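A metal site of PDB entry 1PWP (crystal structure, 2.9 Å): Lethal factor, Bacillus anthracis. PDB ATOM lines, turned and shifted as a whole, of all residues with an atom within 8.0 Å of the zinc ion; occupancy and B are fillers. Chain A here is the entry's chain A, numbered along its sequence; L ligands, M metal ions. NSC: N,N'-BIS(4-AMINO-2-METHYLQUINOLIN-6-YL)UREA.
The zinc ion is bound by OE1 of Glu 735, NE2 of His 690 and NE2 of His 686.
Slightly farther from the zinc ion lies OE2 of Glu 735 (2.8 Å).
Residues that only touch the zinc ion: Tyr 728 (3.1 Å).
Four residues have an atom within 4 Å of the zinc ion: His 686, His 690, Tyr 728 and Glu 735.
The nearest printed residue that does not touch the zinc ion is Glu 687 (4.3 Å).
OH of Tyr 728 sits at hydrogen-bond distance from N13 of the ligand, at 3.2 Å.
OE1 of Glu 735 lies close to OH of Tyr 728 (2.7 Å).
The side-chain amide oxygen of Asn 732 lies within hydrogen-bond range of the backbone NH of Glu 735, at 2.8 Å.
OE1 of Glu 739 sits at hydrogen-bond distance from ND1 of His 686 (2.7 Å).
The side-chain hydroxyl of Thr 731 sits at hydrogen-bond distance from the backbone carbonyl oxygen of Tyr 728 (2.8 Å).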
ATOM      1  N   SER A 655      11.812 -36.343  -4.281  1.00  0.00           N
ATOM      2  CA  SER A 655      10.953 -35.182  -4.226  1.00  0.00           C
ATOM      3  C   SER A 655      10.515 -34.818  -5.626  1.00  0.00           C
ATOM      4  O   SER A 655      10.831 -35.511  -6.575  1.00  0.00           O
ATOM      5  CB  SER A 655      11.691 -34.025  -3.607  1.00  0.00           C
ATOM      6  OG  SER A 655      12.864 -33.742  -4.347  1.00  0.00           O
ATOM      7  N   GLY A 657      11.536 -32.512  -7.617  1.00  0.00           N
ATOM      8  CA  GLY A 657      12.653 -32.285  -8.503  1.00  0.00           C
ATOM      9  C   GLY A 657      13.925 -32.394  -7.702  1.00  0.00           C
ATOM     10  O   GLY A 657      13.880 -32.514  -6.473  1.00  0.00           O
ATOM     11  N   LEU A 658      15.052 -32.332  -8.394  1.00  0.00           N
ATOM     12  CA  LEU A 658      16.351 -32.429  -7.756  1.00  0.00           C
ATOM     13  C   LEU A 658      17.418 -32.178  -8.772  1.00  0.00           C
ATOM     14  O   LEU A 658      17.267 -32.539  -9.942  1.00  0.00           O
ATOM     15  CB  LEU A 658      16.549 -33.834  -7.186  1.00  0.00           C
ATOM     16  CG  LEU A 658      17.916 -34.116  -6.544  1.00  0.00           C
ATOM     17  CD1 LEU A 658      17.899 -33.609  -5.100  1.00  0.00           C
ATOM     18  CD2 LEU A 658      18.214 -35.611  -6.584  1.00  0.00           C
ATOM     19  N   TYR A 659      18.485 -31.529  -8.331  1.00  0.00           N
ATOM     20  CA  TYR A 659      19.638 -31.261  -9.195  1.00  0.00           C
ATOM     21  C   TYR A 659      20.829 -31.976  -8.562  1.00  0.00           C
ATOM     22  O   TYR A 659      21.062 -31.884  -7.361  1.00  0.00           O
ATOM     23  CB  TYR A 659      19.919 -29.766  -9.292  1.00  0.00           C
ATOM     24  CG  TYR A 659      21.119 -29.476 -10.141  1.00  0.00           C
ATOM     25  CD1 TYR A 659      21.150 -29.831 -11.486  1.00  0.00           C
ATOM     26  CD2 TYR A 659      22.251 -28.864  -9.601  1.00  0.00           C
ATOM     27  CE1 TYR A 659      22.259 -29.588 -12.281  1.00  0.00           C
ATOM     28  CE2 TYR A 659      23.376 -28.628 -10.380  1.00  0.00           C
ATOM     29  CZ  TYR A 659      23.382 -28.991 -11.716  1.00  0.00           C
ATOM     30  OH  TYR A 659      24.501 -28.773 -12.484  1.00  0.00           O
ATOM     31  N   LEU A 677       5.401 -25.516  -5.132  1.00  0.00           N
ATOM     32  CA  LEU A 677       5.382 -25.421  -6.588  1.00  0.00           C
ATOM     33  C   LEU A 677       4.001 -25.795  -7.126  1.00  0.00           C
ATOM     34  O   LEU A 677       3.538 -26.913  -6.907  1.00  0.00           O
ATOM     35  CB  LEU A 677       6.450 -26.345  -7.174  1.00  0.00           C
ATOM     36  CG  LEU A 677       7.767 -26.334  -6.400  1.00  0.00           C
ATOM     37  CD1 LEU A 677       8.662 -27.481  -6.861  1.00  0.00           C
ATOM     38  CD2 LEU A 677       8.456 -24.991  -6.591  1.00  0.00           C
ATOM     39  N   GLY A 683       8.596 -26.274 -11.010  1.00  0.00           N
ATOM     40  CA  GLY A 683       9.534 -27.211 -10.438  1.00  0.00           C
ATOM     41  C   GLY A 683      10.813 -27.324 -11.225  1.00  0.00           C
ATOM     42  O   GLY A 683      11.903 -27.214 -10.671  1.00  0.00           O
ATOM     43  N   HIS A 686      12.930 -24.236 -11.065  1.00  0.00           N
ATOM     44  CA  HIS A 686      13.531 -24.137  -9.746  1.00  0.00           C
ATOM     45  C   HIS A 686      14.839 -24.916  -9.718  1.00  0.00           C
ATOM     46  O   HIS A 686      15.836 -24.464  -9.127  1.00  0.00           O
ATOM     47  CB  HIS A 686      12.585 -24.727  -8.713  1.00  0.00           C
ATOM     48  CG  HIS A 686      13.222 -24.911  -7.388  1.00  0.00           C
ATOM     49  ND1 HIS A 686      13.024 -24.041  -6.337  1.00  0.00           N
ATOM     50  CD2 HIS A 686      14.078 -25.864  -6.935  1.00  0.00           C
ATOM     51  CE1 HIS A 686      13.730 -24.444  -5.297  1.00  0.00           C
ATOM     52  NE2 HIS A 686      14.389 -25.540  -5.630  1.00  0.00           N
ATOM     53  N   GLU A 687      14.836 -26.096 -10.336  1.00  0.00           N
ATOM     54  CA  GLU A 687      16.027 -26.932 -10.373  1.00  0.00           C
ATOM     55  C   GLU A 687      17.039 -26.371 -11.340  1.00  0.00           C
ATOM     56  O   GLU A 687      18.234 -26.628 -11.202  1.00  0.00           O
ATOM     57  CB  GLU A 687      15.660 -28.349 -10.799  1.00  0.00           C
ATOM     58  CG  GLU A 687      14.580 -28.955  -9.939  1.00  0.00           C
ATOM     59  CD  GLU A 687      15.016 -29.178  -8.511  1.00  0.00           C
ATOM     60  OE1 GLU A 687      14.140 -29.473  -7.670  1.00  0.00           O
ATOM     61  OE2 GLU A 687      16.225 -29.059  -8.214  1.00  0.00           O
ATOM     62  N   PHE A 688      16.589 -25.609 -12.327  1.00  0.00           N
ATOM     63  CA  PHE A 688      17.542 -25.010 -13.253  1.00  0.00           C
ATOM     64  C   PHE A 688      18.275 -23.902 -12.484  1.00  0.00           C
ATOM     65  O   PHE A 688      19.386 -23.507 -12.846  1.00  0.00           O
ATOM     66  CB  PHE A 688      16.824 -24.416 -14.474  1.00  0.00           C
ATOM     67  CG  PHE A 688      17.747 -24.099 -15.606  1.00  0.00           C
ATOM     68  CD1 PHE A 688      18.214 -25.111 -16.427  1.00  0.00           C
ATOM     69  CD2 PHE A 688      18.198 -22.813 -15.822  1.00  0.00           C
ATOM     70  CE1 PHE A 688      19.118 -24.852 -17.449  1.00  0.00           C
ATOM     71  CE2 PHE A 688      19.104 -22.541 -16.832  1.00  0.00           C
ATOM     72  CZ  PHE A 688      19.565 -23.562 -17.652  1.00  0.00           C
ATOM     73  N   GLY A 689      17.648 -23.405 -11.437  1.00  0.00           N
ATOM     74  CA  GLY A 689      18.275 -22.383 -10.622  1.00  0.00           C
ATOM     75  C   GLY A 689      19.530 -22.961 -10.000  1.00  0.00           C
ATOM     76  O   GLY A 689      20.596 -22.357 -10.045  1.00  0.00           O
ATOM     77  N   HIS A 690      19.405 -24.154  -9.420  1.00  0.00           N
ATOM     78  CA  HIS A 690      20.534 -24.826  -8.810  1.00  0.00           C
ATOM     79  C   HIS A 690      21.631 -25.052  -9.851  1.00  0.00           C
ATOM     80  O   HIS A 690      22.819 -24.999  -9.542  1.00  0.00           O
ATOM     81  CB  HIS A 690      20.098 -26.170  -8.236  1.00  0.00           C
ATOM     82  CG  HIS A 690      19.182 -26.064  -7.068  1.00  0.00           C
ATOM     83  ND1 HIS A 690      19.625 -25.837  -5.787  1.00  0.00           N
ATOM     84  CD2 HIS A 690      17.836 -26.201  -6.980  1.00  0.00           C
ATOM     85  CE1 HIS A 690      18.599 -25.846  -4.956  1.00  0.00           C
ATOM     86  NE2 HIS A 690      17.502 -26.061  -5.652  1.00  0.00           N
ATOM     87  N   TYR A 728       9.654 -22.534   1.650  1.00  0.00           N
ATOM     88  CA  TYR A 728      10.626 -23.479   1.125  1.00  0.00           C
ATOM     89  C   TYR A 728      11.928 -22.757   0.829  1.00  0.00           C
ATOM     90  O   TYR A 728      13.012 -23.271   1.105  1.00  0.00           O
ATOM     91  CB  TYR A 728      10.089 -24.134  -0.156  1.00  0.00           C
ATOM     92  CG  TYR A 728      11.045 -25.088  -0.828  1.00  0.00           C
ATOM     93  CD1 TYR A 728      11.733 -26.066  -0.099  1.00  0.00           C
ATOM     94  CD2 TYR A 728      11.241 -25.056  -2.209  1.00  0.00           C
ATOM     95  CE1 TYR A 728      12.585 -26.980  -0.722  1.00  0.00           C
ATOM     96  CE2 TYR A 728      12.083 -25.955  -2.848  1.00  0.00           C
ATOM     97  CZ  TYR A 728      12.750 -26.919  -2.098  1.00  0.00           C
ATOM     98  OH  TYR A 728      13.584 -27.813  -2.733  1.00  0.00           O
ATOM     99  N   THR A 731      14.609 -22.475   3.558  1.00  0.00           N
ATOM    100  CA  THR A 731      15.376 -23.644   3.990  1.00  0.00           C
ATOM    101  C   THR A 731      16.879 -23.397   4.111  1.00  0.00           C
ATOM    102  O   THR A 731      17.509 -23.776   5.099  1.00  0.00           O
ATOM    103  CB  THR A 731      15.147 -24.832   3.030  1.00  0.00           C
ATOM    104  OG1 THR A 731      13.760 -25.198   3.031  1.00  0.00           O
ATOM    105  CG2 THR A 731      15.980 -26.038   3.462  1.00  0.00           C
ATOM    106  N   ASN A 732      17.463 -22.767   3.094  1.00  0.00           N
ATOM    107  CA  ASN A 732      18.887 -22.458   3.082  1.00  0.00           C
ATOM    108  C   ASN A 732      19.220 -21.600   1.870  1.00  0.00           C
ATOM    109  O   ASN A 732      18.375 -21.387   1.009  1.00  0.00           O
ATOM    110  CB  ASN A 732      19.700 -23.742   3.032  1.00  0.00           C
ATOM    111  CG  ASN A 732      19.599 -24.435   1.704  1.00  0.00           C
ATOM    112  OD1 ASN A 732      19.881 -23.850   0.668  1.00  0.00           O
ATOM    113  ND2 ASN A 732      19.190 -25.686   1.732  1.00  0.00           N
ATOM    114  N   ALA A 734      21.214 -22.122  -0.889  1.00  0.00           N
ATOM    115  CA  ALA A 734      21.117 -22.759  -2.201  1.00  0.00           C
ATOM    116  C   ALA A 734      19.675 -22.805  -2.674  1.00  0.00           C
ATOM    117  O   ALA A 734      19.385 -22.552  -3.844  1.00  0.00           O
ATOM    118  CB  ALA A 734      21.703 -24.161  -2.157  1.00  0.00           C
ATOM    119  N   GLU A 735      18.771 -23.123  -1.758  1.00  0.00           N
ATOM    120  CA  GLU A 735      17.348 -23.207  -2.069  1.00  0.00           C
ATOM    121  C   GLU A 735      16.730 -21.811  -2.221  1.00  0.00           C
ATOM    122  O   GLU A 735      15.932 -21.571  -3.121  1.00  0.00           O
ATOM    123  CB  GLU A 735      16.625 -23.981  -0.977  1.00  0.00           C
ATOM    124  CG  GLU A 735      17.096 -25.420  -0.811  1.00  0.00           C
ATOM    125  CD  GLU A 735      16.827 -26.262  -2.042  1.00  0.00           C
ATOM    126  OE1 GLU A 735      15.689 -26.193  -2.554  1.00  0.00           O
ATOM    127  OE2 GLU A 735      17.732 -26.992  -2.502  1.00  0.00           O
ATOM    128  N   PHE A 736      17.110 -20.908  -1.326  1.00  0.00           N
ATOM    129  CA  PHE A 736      16.603 -19.548  -1.365  1.00  0.00           C
ATOM    130  C   PHE A 736      16.932 -18.934  -2.724  1.00  0.00           C
ATOM    131  O   PHE A 736      16.102 -18.253  -3.329  1.00  0.00           O
ATOM    132  CB  PHE A 736      17.220 -18.714  -0.240  1.00  0.00           C
ATOM    133  CG  PHE A 736      16.780 -17.272  -0.244  1.00  0.00           C
ATOM    134  CD1 PHE A 736      15.427 -16.955  -0.210  1.00  0.00           C
ATOM    135  CD2 PHE A 736      17.710 -16.242  -0.312  1.00  0.00           C
ATOM    136  CE1 PHE A 736      15.004 -15.631  -0.267  1.00  0.00           C
ATOM    137  CE2 PHE A 736      17.297 -14.924  -0.364  1.00  0.00           C
ATOM    138  CZ  PHE A 736      15.944 -14.619  -0.342  1.00  0.00           C
ATOM    139  N   PHE A 737      18.155 -19.186  -3.198  1.00  0.00           N
ATOM    140  CA  PHE A 737      18.608 -18.664  -4.478  1.00  0.00           C
ATOM    141  C   PHE A 737      17.750 -19.262  -5.582  1.00  0.00           C
ATOM    142  O   PHE A 737      17.355 -18.571  -6.524  1.00  0.00           O
ATOM    143  CB  PHE A 737      20.073 -19.044  -4.720  1.00  0.00           C
ATOM    144  CG  PHE A 737      20.609 -18.622  -6.069  1.00  0.00           C
ATOM    145  CD1 PHE A 737      21.152 -17.359  -6.251  1.00  0.00           C
ATOM    146  CD2 PHE A 737      20.573 -19.494  -7.151  1.00  0.00           C
ATOM    147  CE1 PHE A 737      21.667 -16.980  -7.486  1.00  0.00           C
ATOM    148  CE2 PHE A 737      21.080 -19.123  -8.395  1.00  0.00           C
ATOM    149  CZ  PHE A 737      21.631 -17.862  -8.558  1.00  0.00           C
ATOM    150  N   ALA A 738      17.471 -20.559  -5.440  1.00  0.00           N
ATOM    151  CA  ALA A 738      16.683 -21.294  -6.415  1.00  0.00           C
ATOM    152  C   ALA A 738      15.222 -20.858  -6.463  1.00  0.00           C
ATOM    153  O   ALA A 738      14.643 -20.736  -7.547  1.00  0.00           O
ATOM    154  CB  ALA A 738      16.780 -22.780  -6.128  1.00  0.00           C
ATOM    155  N   GLU A 739      14.622 -20.626  -5.295  1.00  0.00           N
ATOM    156  CA  GLU A 739      13.235 -20.175  -5.263  1.00  0.00           C
ATOM    157  C   GLU A 739      13.131 -18.764  -5.829  1.00  0.00           C
ATOM    158  O   GLU A 739      12.166 -18.431  -6.516  1.00  0.00           O
ATOM    159  CB  GLU A 739      12.690 -20.217  -3.833  1.00  0.00           C
ATOM    160  CG  GLU A 739      11.953 -21.513  -3.463  1.00  0.00           C
ATOM    161  CD  GLU A 739      10.826 -21.858  -4.445  1.00  0.00           C
ATOM    162  OE1 GLU A 739      11.116 -22.328  -5.564  1.00  0.00           O
ATOM    163  OE2 GLU A 739       9.649 -21.657  -4.094  1.00  0.00           O
HETATM  164  C12 NSC L   1      14.777 -31.787  -0.876  1.00  0.00           C
HETATM  165  C3  NSC L   1      13.957 -32.335   0.130  1.00  0.00           C
HETATM  166  C2  NSC L   1      14.521 -32.922   1.286  1.00  0.00           C
HETATM  167  N1  NSC L   1      15.843 -32.948   1.452  1.00  0.00           N
HETATM  168  C7  NSC L   1      13.671 -33.492   2.259  1.00  0.00           C
HETATM  169  C6  NSC L   1      12.280 -33.453   2.069  1.00  0.00           C
HETATM  170  C8  NSC L   1      11.349 -34.073   3.115  1.00  0.00           C
HETATM  171  N5  NSC L   1      11.752 -32.882   0.951  1.00  0.00           N
HETATM  172  C4  NSC L   1      12.547 -32.327  -0.011  1.00  0.00           C
HETATM  173  C9  NSC L   1      11.961 -31.762  -1.160  1.00  0.00           C
HETATM  174  C10 NSC L   1      12.776 -31.222  -2.166  1.00  0.00           C
HETATM  175  C11 NSC L   1      14.187 -31.221  -2.035  1.00  0.00           C
HETATM  176  N13 NSC L   1      14.930 -30.712  -3.046  1.00  0.00           N
HETATM  177  C14 NSC L   1      16.267 -30.635  -3.104  1.00  0.00           C
HETATM  178  O28 NSC L   1      16.998 -31.055  -2.196  1.00  0.00           O
HETATM  179  N15 NSC L   1      16.769 -30.076  -4.225  1.00  0.00           N
HETATM  180  C16 NSC L   1      18.078 -29.873  -4.519  1.00  0.00           C
HETATM  181  C17 NSC L   1      19.117 -30.103  -3.578  1.00  0.00           C
HETATM  182  C18 NSC L   1      20.450 -29.756  -3.897  1.00  0.00           C
HETATM  183  C24 NSC L   1      21.492 -29.944  -2.975  1.00  0.00           C
HETATM  184  N25 NSC L   1      21.252 -30.488  -1.778  1.00  0.00           N
HETATM  185  C23 NSC L   1      22.799 -29.561  -3.312  1.00  0.00           C
HETATM  186  C21 NSC L   1      23.050 -28.985  -4.576  1.00  0.00           C
HETATM  187  C20 NSC L   1      24.470 -28.567  -4.958  1.00  0.00           C
HETATM  188  N22 NSC L   1      22.022 -28.811  -5.452  1.00  0.00           N
HETATM  189  C19 NSC L   1      20.746 -29.180  -5.148  1.00  0.00           C
HETATM  190  C26 NSC L   1      19.718 -28.956  -6.083  1.00  0.00           C
HETATM  191  C27 NSC L   1      18.391 -29.294  -5.765  1.00  0.00           C
HETATM  192 ZN    ZN M   1      15.888 -26.874  -4.545  1.00  0.00          ZN
